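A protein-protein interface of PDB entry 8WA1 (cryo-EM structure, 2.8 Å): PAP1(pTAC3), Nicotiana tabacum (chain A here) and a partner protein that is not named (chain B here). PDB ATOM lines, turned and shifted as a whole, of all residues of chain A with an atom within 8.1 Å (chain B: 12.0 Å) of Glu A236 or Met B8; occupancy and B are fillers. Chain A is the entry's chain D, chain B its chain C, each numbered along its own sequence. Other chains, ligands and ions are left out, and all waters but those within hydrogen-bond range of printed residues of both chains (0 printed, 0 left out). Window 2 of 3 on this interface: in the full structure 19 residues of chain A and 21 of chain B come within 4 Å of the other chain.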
ATOM      1  N   TYR A 212     -18.621 -32.862  14.287  1.00  0.00           N
ATOM      2  CA  TYR A 212     -17.641 -31.795  14.477  1.00  0.00           C
ATOM      3  C   TYR A 212     -18.266 -30.429  14.230  1.00  0.00           C
ATOM      4  O   TYR A 212     -18.142 -29.515  15.056  1.00  0.00           O
ATOM      5  CB  TYR A 212     -16.452 -32.006  13.539  1.00  0.00           C
ATOM      6  CG  TYR A 212     -15.532 -33.146  13.912  1.00  0.00           C
ATOM      7  CD1 TYR A 212     -14.963 -33.224  15.175  1.00  0.00           C
ATOM      8  CD2 TYR A 212     -15.226 -34.142  12.994  1.00  0.00           C
ATOM      9  CE1 TYR A 212     -14.117 -34.264  15.513  1.00  0.00           C
ATOM     10  CE2 TYR A 212     -14.384 -35.186  13.324  1.00  0.00           C
ATOM     11  CZ  TYR A 212     -13.832 -35.242  14.585  1.00  0.00           C
ATOM     12  OH  TYR A 212     -12.992 -36.278  14.920  1.00  0.00           O
ATOM     13  N   LEU A 229     -12.180 -24.779  20.460  1.00  0.00           N
ATOM     14  CA  LEU A 229     -10.796 -24.913  20.017  1.00  0.00           C
ATOM     15  C   LEU A 229     -10.261 -26.311  20.304  1.00  0.00           C
ATOM     16  O   LEU A 229      -9.493 -26.866  19.510  1.00  0.00           O
ATOM     17  CB  LEU A 229      -9.926 -23.851  20.688  1.00  0.00           C
ATOM     18  CG  LEU A 229      -8.476 -23.746  20.215  1.00  0.00           C
ATOM     19  CD1 LEU A 229      -8.418 -23.463  18.722  1.00  0.00           C
ATOM     20  CD2 LEU A 229      -7.734 -22.673  20.995  1.00  0.00           C
ATOM     21  N   THR A 230     -10.662 -26.900  21.433  1.00  0.00           N
ATOM     22  CA  THR A 230     -10.232 -28.260  21.744  1.00  0.00           C
ATOM     23  C   THR A 230     -10.803 -29.261  20.745  1.00  0.00           C
ATOM     24  O   THR A 230     -10.099 -30.176  20.299  1.00  0.00           O
ATOM     25  CB  THR A 230     -10.644 -28.630  23.169  1.00  0.00           C
ATOM     26  OG1 THR A 230     -10.161 -27.635  24.079  1.00  0.00           O
ATOM     27  CG2 THR A 230     -10.064 -29.982  23.556  1.00  0.00           C
ATOM     28  N   ILE A 231     -12.076 -29.100  20.377  1.00  0.00           N
ATOM     29  CA  ILE A 231     -12.686 -29.985  19.388  1.00  0.00           C
ATOM     30  C   ILE A 231     -12.028 -29.798  18.028  1.00  0.00           C
ATOM     31  O   ILE A 231     -11.825 -30.763  17.283  1.00  0.00           O
ATOM     32  CB  ILE A 231     -14.207 -29.748  19.327  1.00  0.00           C
ATOM     33  CG1 ILE A 231     -14.861 -30.180  20.640  1.00  0.00           C
ATOM     34  CG2 ILE A 231     -14.826 -30.497  18.156  1.00  0.00           C
ATOM     35  CD1 ILE A 231     -16.341 -29.889  20.710  1.00  0.00           C
ATOM     36  N   ALA A 232     -11.668 -28.557  17.686  1.00  0.00           N
ATOM     37  CA  ALA A 232     -10.974 -28.316  16.425  1.00  0.00           C
ATOM     38  C   ALA A 232      -9.599 -28.975  16.417  1.00  0.00           C
ATOM     39  O   ALA A 232      -9.183 -29.554  15.405  1.00  0.00           O
ATOM     40  CB  ALA A 232     -10.855 -26.815  16.170  1.00  0.00           C
ATOM     41  N   TYR A 233      -8.878 -28.894  17.538  1.00  0.00           N
ATOM     42  CA  TYR A 233      -7.583 -29.561  17.639  1.00  0.00           C
ATOM     43  C   TYR A 233      -7.728 -31.072  17.521  1.00  0.00           C
ATOM     44  O   TYR A 233      -6.931 -31.725  16.838  1.00  0.00           O
ATOM     45  CB  TYR A 233      -6.901 -29.189  18.954  1.00  0.00           C
ATOM     46  CG  TYR A 233      -6.251 -27.826  18.948  1.00  0.00           C
ATOM     47  CD1 TYR A 233      -5.746 -27.282  17.775  1.00  0.00           C
ATOM     48  CD2 TYR A 233      -6.142 -27.083  20.114  1.00  0.00           C
ATOM     49  CE1 TYR A 233      -5.149 -26.037  17.765  1.00  0.00           C
ATOM     50  CE2 TYR A 233      -5.547 -25.836  20.114  1.00  0.00           C
ATOM     51  CZ  TYR A 233      -5.053 -25.318  18.938  1.00  0.00           C
ATOM     52  OH  TYR A 233      -4.460 -24.076  18.932  1.00  0.00           O
ATOM     53  N   GLU A 234      -8.738 -31.644  18.179  1.00  0.00           N
ATOM     54  CA  GLU A 234      -8.966 -33.083  18.073  1.00  0.00           C
ATOM     55  C   GLU A 234      -9.328 -33.482  16.647  1.00  0.00           C
ATOM     56  O   GLU A 234      -8.896 -34.534  16.160  1.00  0.00           O
ATOM     57  CB  GLU A 234     -10.061 -33.514  19.048  1.00  0.00           C
ATOM     58  CG  GLU A 234      -9.638 -33.489  20.508  1.00  0.00           C
ATOM     59  CD  GLU A 234      -8.644 -34.585  20.847  1.00  0.00           C
ATOM     60  OE1 GLU A 234      -8.577 -35.583  20.100  1.00  0.00           O
ATOM     61  OE2 GLU A 234      -7.930 -34.446  21.862  1.00  0.00           O
ATOM     62  N   MET A 235     -10.117 -32.652  15.961  1.00  0.00           N
ATOM     63  CA  MET A 235     -10.462 -32.930  14.571  1.00  0.00           C
ATOM     64  C   MET A 235      -9.227 -32.910  13.683  1.00  0.00           C
ATOM     65  O   MET A 235      -9.036 -33.805  12.852  1.00  0.00           O
ATOM     66  CB  MET A 235     -11.487 -31.912  14.072  1.00  0.00           C
ATOM     67  CG  MET A 235     -11.823 -32.056  12.598  1.00  0.00           C
ATOM     68  SD  MET A 235     -12.246 -30.481  11.834  1.00  0.00           S
ATOM     69  CE  MET A 235     -13.527 -29.913  12.943  1.00  0.00           C
ATOM     70  N   GLU A 236      -8.379 -31.891  13.838  1.00  0.00           N
ATOM     71  CA  GLU A 236      -7.169 -31.817  13.024  1.00  0.00           C
ATOM     72  C   GLU A 236      -6.211 -32.956  13.353  1.00  0.00           C
ATOM     73  O   GLU A 236      -5.478 -33.431  12.478  1.00  0.00           O
ATOM     74  CB  GLU A 236      -6.489 -30.463  13.210  1.00  0.00           C
ATOM     75  CG  GLU A 236      -7.252 -29.314  12.577  1.00  0.00           C
ATOM     76  CD  GLU A 236      -6.393 -28.085  12.372  1.00  0.00           C
ATOM     77  OE1 GLU A 236      -5.394 -27.925  13.103  1.00  0.00           O
ATOM     78  OE2 GLU A 236      -6.714 -27.281  11.471  1.00  0.00           O
ATOM     79  N   ALA A 237      -6.204 -33.409  14.608  1.00  0.00           N
ATOM     80  CA  ALA A 237      -5.394 -34.569  14.965  1.00  0.00           C
ATOM     81  C   ALA A 237      -5.948 -35.840  14.332  1.00  0.00           C
ATOM     82  O   ALA A 237      -5.186 -36.737  13.955  1.00  0.00           O
ATOM     83  CB  ALA A 237      -5.320 -34.713  16.484  1.00  0.00           C
ATOM     84  N   ALA A 238      -7.272 -35.932  14.207  1.00  0.00           N
ATOM     85  CA  ALA A 238      -7.910 -37.095  13.604  1.00  0.00           C
ATOM     86  C   ALA A 238      -7.707 -37.175  12.096  1.00  0.00           C
ATOM     87  O   ALA A 238      -8.084 -38.188  11.496  1.00  0.00           O
ATOM     88  CB  ALA A 238      -9.405 -37.095  13.923  1.00  0.00           C
ATOM     89  N   GLY A 239      -7.125 -36.153  11.472  1.00  0.00           N
ATOM     90  CA  GLY A 239      -6.849 -36.170  10.052  1.00  0.00           C
ATOM     91  C   GLY A 239      -7.665 -35.204   9.219  1.00  0.00           C
ATOM     92  O   GLY A 239      -7.267 -34.905   8.086  1.00  0.00           O
ATOM     93  N   ARG A 240      -8.786 -34.709   9.736  1.00  0.00           N
ATOM     94  CA  ARG A 240      -9.617 -33.758   9.007  1.00  0.00           C
ATOM     95  C   ARG A 240      -9.144 -32.341   9.303  1.00  0.00           C
ATOM     96  O   ARG A 240      -9.120 -31.919  10.463  1.00  0.00           O
ATOM     97  CB  ARG A 240     -11.090 -33.913   9.383  1.00  0.00           C
ATOM     98  CG  ARG A 240     -12.007 -32.974   8.612  1.00  0.00           C
ATOM     99  CD  ARG A 240     -13.353 -32.796   9.294  1.00  0.00           C
ATOM    100  NE  ARG A 240     -14.212 -31.876   8.554  1.00  0.00           N
ATOM    101  CZ  ARG A 240     -15.337 -31.353   9.029  1.00  0.00           C
ATOM    102  NH1 ARG A 240     -15.744 -31.653  10.255  1.00  0.00           N
ATOM    103  NH2 ARG A 240     -16.055 -30.526   8.282  1.00  0.00           N
ATOM    104  N   MET A 241      -8.774 -31.609   8.257  1.00  0.00           N
ATOM    105  CA  MET A 241      -8.345 -30.231   8.420  1.00  0.00           C
ATOM    106  C   MET A 241      -9.551 -29.320   8.638  1.00  0.00           C
ATOM    107  O   MET A 241     -10.707 -29.713   8.459  1.00  0.00           O
ATOM    108  CB  MET A 241      -7.539 -29.774   7.205  1.00  0.00           C
ATOM    109  CG  MET A 241      -6.297 -30.608   6.941  1.00  0.00           C
ATOM    110  SD  MET A 241      -5.182 -30.654   8.358  1.00  0.00           S
ATOM    111  CE  MET A 241      -3.897 -31.740   7.745  1.00  0.00           C
ATOM    112  N   ALA A 242      -9.268 -28.083   9.033  1.00  0.00           N
ATOM    113  CA  ALA A 242     -10.298 -27.094   9.312  1.00  0.00           C
ATOM    114  C   ALA A 242     -10.517 -26.207   8.095  1.00  0.00           C
ATOM    115  O   ALA A 242      -9.570 -25.873   7.375  1.00  0.00           O
ATOM    116  CB  ALA A 242      -9.919 -26.238  10.522  1.00  0.00           C
ATOM    117  N   THR A 243     -11.770 -25.827   7.870  1.00  0.00           N
ATOM    118  CA  THR A 243     -12.156 -24.975   6.757  1.00  0.00           C
ATOM    119  C   THR A 243     -12.506 -23.582   7.273  1.00  0.00           C
ATOM    120  O   THR A 243     -12.417 -23.294   8.470  1.00  0.00           O
ATOM    121  CB  THR A 243     -13.330 -25.587   5.989  1.00  0.00           C
ATOM    122  OG1 THR A 243     -14.448 -25.749   6.871  1.00  0.00           O
ATOM    123  CG2 THR A 243     -12.941 -26.942   5.418  1.00  0.00           C
ATOM    124  N   HIS A 246     -15.153 -23.245  10.332  1.00  0.00           N
ATOM    125  CA  HIS A 246     -14.706 -23.375  11.716  1.00  0.00           C
ATOM    126  C   HIS A 246     -13.947 -22.135  12.171  1.00  0.00           C
ATOM    127  O   HIS A 246     -14.114 -21.679  13.309  1.00  0.00           O
ATOM    128  CB  HIS A 246     -13.837 -24.623  11.866  1.00  0.00           C
ATOM    129  CG  HIS A 246     -14.462 -25.863  11.306  1.00  0.00           C
ATOM    130  ND1 HIS A 246     -13.719 -26.935  10.857  1.00  0.00           N
ATOM    131  CD2 HIS A 246     -15.759 -26.202  11.121  1.00  0.00           C
ATOM    132  CE1 HIS A 246     -14.532 -27.878  10.417  1.00  0.00           C
ATOM    133  NE2 HIS A 246     -15.776 -27.459  10.568  1.00  0.00           N
ATOM    134  N   PHE A 247     -13.113 -21.573  11.295  1.00  0.00           N
ATOM    135  CA  PHE A 247     -12.365 -20.374  11.658  1.00  0.00           C
ATOM    136  C   PHE A 247     -13.292 -19.181  11.854  1.00  0.00           C
ATOM    137  O   PHE A 247     -13.076 -18.364  12.756  1.00  0.00           O
ATOM    138  CB  PHE A 247     -11.310 -20.069  10.597  1.00  0.00           C
ATOM    139  CG  PHE A 247     -10.126 -20.989  10.638  1.00  0.00           C
ATOM    140  CD1 PHE A 247      -9.205 -20.905  11.667  1.00  0.00           C
ATOM    141  CD2 PHE A 247      -9.927 -21.928   9.642  1.00  0.00           C
ATOM    142  CE1 PHE A 247      -8.112 -21.747  11.707  1.00  0.00           C
ATOM    143  CE2 PHE A 247      -8.836 -22.772   9.676  1.00  0.00           C
ATOM    144  CZ  PHE A 247      -7.928 -22.681  10.709  1.00  0.00           C
ATOM    145  N   ASN A 269      -3.434 -16.840  10.023  1.00  0.00           N
ATOM    146  CA  ASN A 269      -3.427 -18.276   9.769  1.00  0.00           C
ATOM    147  C   ASN A 269      -4.280 -18.614   8.552  1.00  0.00           C
ATOM    148  O   ASN A 269      -3.912 -19.470   7.739  1.00  0.00           O
ATOM    149  CB  ASN A 269      -3.922 -19.027  11.006  1.00  0.00           C
ATOM    150  CG  ASN A 269      -3.619 -20.515  10.953  1.00  0.00           C
ATOM    151  OD1 ASN A 269      -3.994 -21.265  11.854  1.00  0.00           O
ATOM    152  ND2 ASN A 269      -2.927 -20.946   9.905  1.00  0.00           N
ATOM    153  N   MET A 270      -5.430 -17.951   8.416  1.00  0.00           N
ATOM    154  CA  MET A 270      -6.307 -18.206   7.276  1.00  0.00           C
ATOM    155  C   MET A 270      -5.714 -17.647   5.986  1.00  0.00           C
ATOM    156  O   MET A 270      -5.762 -18.297   4.936  1.00  0.00           O
ATOM    157  CB  MET A 270      -7.688 -17.599   7.525  1.00  0.00           C
ATOM    158  CG  MET A 270      -8.413 -18.138   8.739  1.00  0.00           C
ATOM    159  SD  MET A 270      -9.996 -17.312   8.975  1.00  0.00           S
ATOM    160  CE  MET A 270     -10.915 -17.959   7.583  1.00  0.00           C
ATOM    161  N   GLY A 273      -2.645 -19.593   4.716  1.00  0.00           N
ATOM    162  CA  GLY A 273      -2.853 -21.024   4.707  1.00  0.00           C
ATOM    163  C   GLY A 273      -3.220 -21.543   3.328  1.00  0.00           C
ATOM    164  O   GLY A 273      -2.967 -20.917   2.298  1.00  0.00           O
ATOM    165  N   GLU A 274      -3.833 -22.723   3.322  1.00  0.00           N
ATOM    166  CA  GLU A 274      -4.264 -23.346   2.081  1.00  0.00           C
ATOM    167  C   GLU A 274      -5.521 -22.663   1.542  1.00  0.00           C
ATOM    168  O   GLU A 274      -6.081 -21.749   2.155  1.00  0.00           O
ATOM    169  CB  GLU A 274      -4.515 -24.840   2.280  1.00  0.00           C
ATOM    170  CG  GLU A 274      -3.256 -25.667   2.499  1.00  0.00           C
ATOM    171  CD  GLU A 274      -2.730 -25.577   3.917  1.00  0.00           C
ATOM    172  OE1 GLU A 274      -3.543 -25.370   4.841  1.00  0.00           O
ATOM    173  OE2 GLU A 274      -1.503 -25.710   4.108  1.00  0.00           O
ATOM    174  N   HIS A 276      -8.547 -23.986   1.040  1.00  0.00           N
ATOM    175  CA  HIS A 276      -9.786 -24.338   1.727  1.00  0.00           C
ATOM    176  C   HIS A 276      -9.984 -23.519   2.994  1.00  0.00           C
ATOM    177  O   HIS A 276     -11.124 -23.291   3.415  1.00  0.00           O
ATOM    178  CB  HIS A 276      -9.808 -25.834   2.048  1.00  0.00           C
ATOM    179  CG  HIS A 276      -8.730 -26.269   2.991  1.00  0.00           C
ATOM    180  ND1 HIS A 276      -7.524 -26.778   2.561  1.00  0.00           N
ATOM    181  CD2 HIS A 276      -8.680 -26.278   4.345  1.00  0.00           C
ATOM    182  CE1 HIS A 276      -6.777 -27.079   3.607  1.00  0.00           C
ATOM    183  NE2 HIS A 276      -7.454 -26.784   4.702  1.00  0.00           N
ATOM    184  N   MET A 277      -8.897 -23.068   3.615  1.00  0.00           N
ATOM    185  CA  MET A 277      -8.970 -22.273   4.834  1.00  0.00           C
ATOM    186  C   MET A 277      -8.760 -20.785   4.589  1.00  0.00           C
ATOM    187  O   MET A 277      -8.579 -20.036   5.555  1.00  0.00           O
ATOM    188  CB  MET A 277      -7.945 -22.779   5.853  1.00  0.00           C
ATOM    189  CG  MET A 277      -6.503 -22.681   5.383  1.00  0.00           C
ATOM    190  SD  MET A 277      -5.332 -23.364   6.572  1.00  0.00           S
ATOM    191  CE  MET A 277      -5.631 -22.311   7.988  1.00  0.00           C
ATOM    192  N   MET B   8      -4.866 -26.598   9.473  1.00  0.00           N
ATOM    193  CA  MET B   8      -3.679 -26.610  10.319  1.00  0.00           C
ATOM    194  C   MET B   8      -3.702 -25.449  11.307  1.00  0.00           C
ATOM    195  O   MET B   8      -2.957 -24.481  11.159  1.00  0.00           O
ATOM    196  CB  MET B   8      -2.411 -26.550   9.466  1.00  0.00           C
ATOM    197  N   ILE B   9      -4.572 -25.551  12.313  1.00  0.00           N
ATOM    198  CA  ILE B   9      -4.652 -24.521  13.341  1.00  0.00           C
ATOM    199  C   ILE B   9      -3.367 -24.534  14.156  1.00  0.00           C
ATOM    200  O   ILE B   9      -2.965 -25.573  14.695  1.00  0.00           O
ATOM    201  CB  ILE B   9      -5.880 -24.737  14.230  1.00  0.00           C
ATOM    202  CG1 ILE B   9      -7.154 -24.759  13.386  1.00  0.00           C
ATOM    203  CG2 ILE B   9      -5.971 -23.646  15.283  1.00  0.00           C
ATOM    204  CD1 ILE B   9      -8.424 -24.862  14.202  1.00  0.00           C
ATOM    205  N   ASP B  10      -2.719 -23.379  14.253  1.00  0.00           N
ATOM    206  CA  ASP B  10      -1.462 -23.280  14.975  1.00  0.00           C
ATOM    207  C   ASP B  10      -1.706 -23.201  16.480  1.00  0.00           C
ATOM    208  O   ASP B  10      -2.803 -22.880  16.946  1.00  0.00           O
ATOM    209  CB  ASP B  10      -0.671 -22.057  14.509  1.00  0.00           C
ATOM    210  CG  ASP B  10      -0.435 -22.052  13.012  1.00  0.00           C
ATOM    211  OD1 ASP B  10      -0.351 -23.148  12.418  1.00  0.00           O
ATOM    212  OD2 ASP B  10      -0.334 -20.953  12.427  1.00  0.00           O
ATOM    213  N   ARG B  11      -0.660 -23.503  17.243  1.00  0.00           N
ATOM    214  CA  ARG B  11      -0.705 -23.404  18.695  1.00  0.00           C
ATOM    215  C   ARG B  11      -0.474 -21.951  19.089  1.00  0.00           C
ATOM    216  O   ARG B  11       0.641 -21.436  18.953  1.00  0.00           O
ATOM    217  CB  ARG B  11       0.342 -24.315  19.334  1.00  0.00           C
ATOM    218  CG  ARG B  11       0.236 -25.773  18.921  1.00  0.00           C
ATOM    219  CD  ARG B  11      -1.019 -26.422  19.479  1.00  0.00           C
ATOM    220  NE  ARG B  11      -1.144 -27.815  19.062  1.00  0.00           N
ATOM    221  CZ  ARG B  11      -2.113 -28.632  19.463  1.00  0.00           C
ATOM    222  NH1 ARG B  11      -2.147 -29.885  19.031  1.00  0.00           N
ATOM    223  NH2 ARG B  11      -3.046 -28.197  20.299  1.00  0.00           N
ATOM    224  N   TYR B  12      -1.523 -21.292  19.572  1.00  0.00           N
ATOM    225  CA  TYR B  12      -1.498 -19.858  19.828  1.00  0.00           C
ATOM    226  C   TYR B  12      -0.927 -19.591  21.214  1.00  0.00           C
ATOM    227  O   TYR B  12      -1.529 -19.973  22.224  1.00  0.00           O
ATOM    228  CB  TYR B  12      -2.900 -19.258  19.706  1.00  0.00           C
ATOM    229  CG  TYR B  12      -3.549 -19.478  18.360  1.00  0.00           C
ATOM    230  CD1 TYR B  12      -3.186 -18.714  17.260  1.00  0.00           C
ATOM    231  CD2 TYR B  12      -4.532 -20.444  18.191  1.00  0.00           C
ATOM    232  CE1 TYR B  12      -3.778 -18.908  16.028  1.00  0.00           C
ATOM    233  CE2 TYR B  12      -5.132 -20.645  16.961  1.00  0.00           C
ATOM    234  CZ  TYR B  12      -4.750 -19.873  15.883  1.00  0.00           C
ATOM    235  OH  TYR B  12      -5.340 -20.067  14.656  1.00  0.00           O
ATOM    236  N   LYS B  13       0.231 -18.939  21.259  1.00  0.00           N
ATOM    237  CA  LYS B  13       0.834 -18.471  22.499  1.00  0.00           C
ATOM    238  C   LYS B  13       0.796 -16.950  22.516  1.00  0.00           C
ATOM    239  O   LYS B  13       1.290 -16.301  21.586  1.00  0.00           O
ATOM    240  CB  LYS B  13       2.271 -18.977  22.646  1.00  0.00           C
ATOM    241  CG  LYS B  13       3.128 -18.813  21.401  1.00  0.00           C
ATOM    242  CD  LYS B  13       4.602 -19.005  21.716  1.00  0.00           C
ATOM    243  CE  LYS B  13       5.094 -17.952  22.696  1.00  0.00           C
ATOM    244  NZ  LYS B  13       6.549 -18.090  22.985  1.00  0.00           N
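N of Met B8 lies within hydrogen-bond range of OE2 of Glu A236 (2.8 Å).
The side-chain hydroxyl of Tyr B12 lies within hydrogen-bond range of the side-chain amide oxygen of Asn A269, at 3.3 Å.
N of Asp B10 lies within hydrogen-bond range of OD1 of Asn A269, at 3.4 Å.
O of Met B8 lies close to OD1 of Asn A269 (3.4 Å).
OE1 of Glu A236 is in hydrogen-bond range of N of Ile B9 (2.6 Å).
The side-chain hydroxyl (OH) of Tyr A233 is in hydrogen-bond range of the backbone carbonyl oxygen (O) of Asp B10 (2.8 Å).
Among the printed residues, pairs that only touch across the chains: Ala A232 with Ile B9 (3.7 Å), Tyr A233 with Ile B9 (3.5 Å), Tyr A233 with Arg B11 (3.3 Å), Tyr A233 with Tyr B12 (3.7 Å), Phe A247 with Ile B9 (3.5 Å) and Asn A269 with Ile B9 (3.6 Å).
Tyr A233 touches four residues of chain B.
Glu A236 touches two residues of chain B.
Ala A237 touches none of the printed residues of chain B.
No residue of chain B comes within 4 Å of Gly A239.
No residue of chain B comes within 4 Å of Met A241.
Ala A242 touches none of the printed residues of chain B.
Thr A243 touches none of the printed residues of chain B.
Glu A274 touches none of the printed residues of chain B.
Met B8 touches two residues of chain A.
Printed residues of chain A within 4 Å of Ile B9: Ala A232 (3.7 Å), Tyr A233 (3.5 Å), Glu A236 (2.6 Å), Phe A247 (3.5 Å) and Asn A269 (3.6 Å).
Of the printed residues of chain A, Arg B11 touches Tyr A233 (3.3 Å).
Of the printed residues of chain A, Tyr B12 touches Tyr A233 (3.7 Å) and Asn A269 (3.3 Å).
Hydrophobic or aromatic side chains of chain A within 4 Å of the printed part of chain B: Ala A232, Tyr A233 and Phe A247.
Of the 6 printed residues of chain B, 5 touch a printed residue of chain A.
Among the printed residues, 12 pairs touch across the chains.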
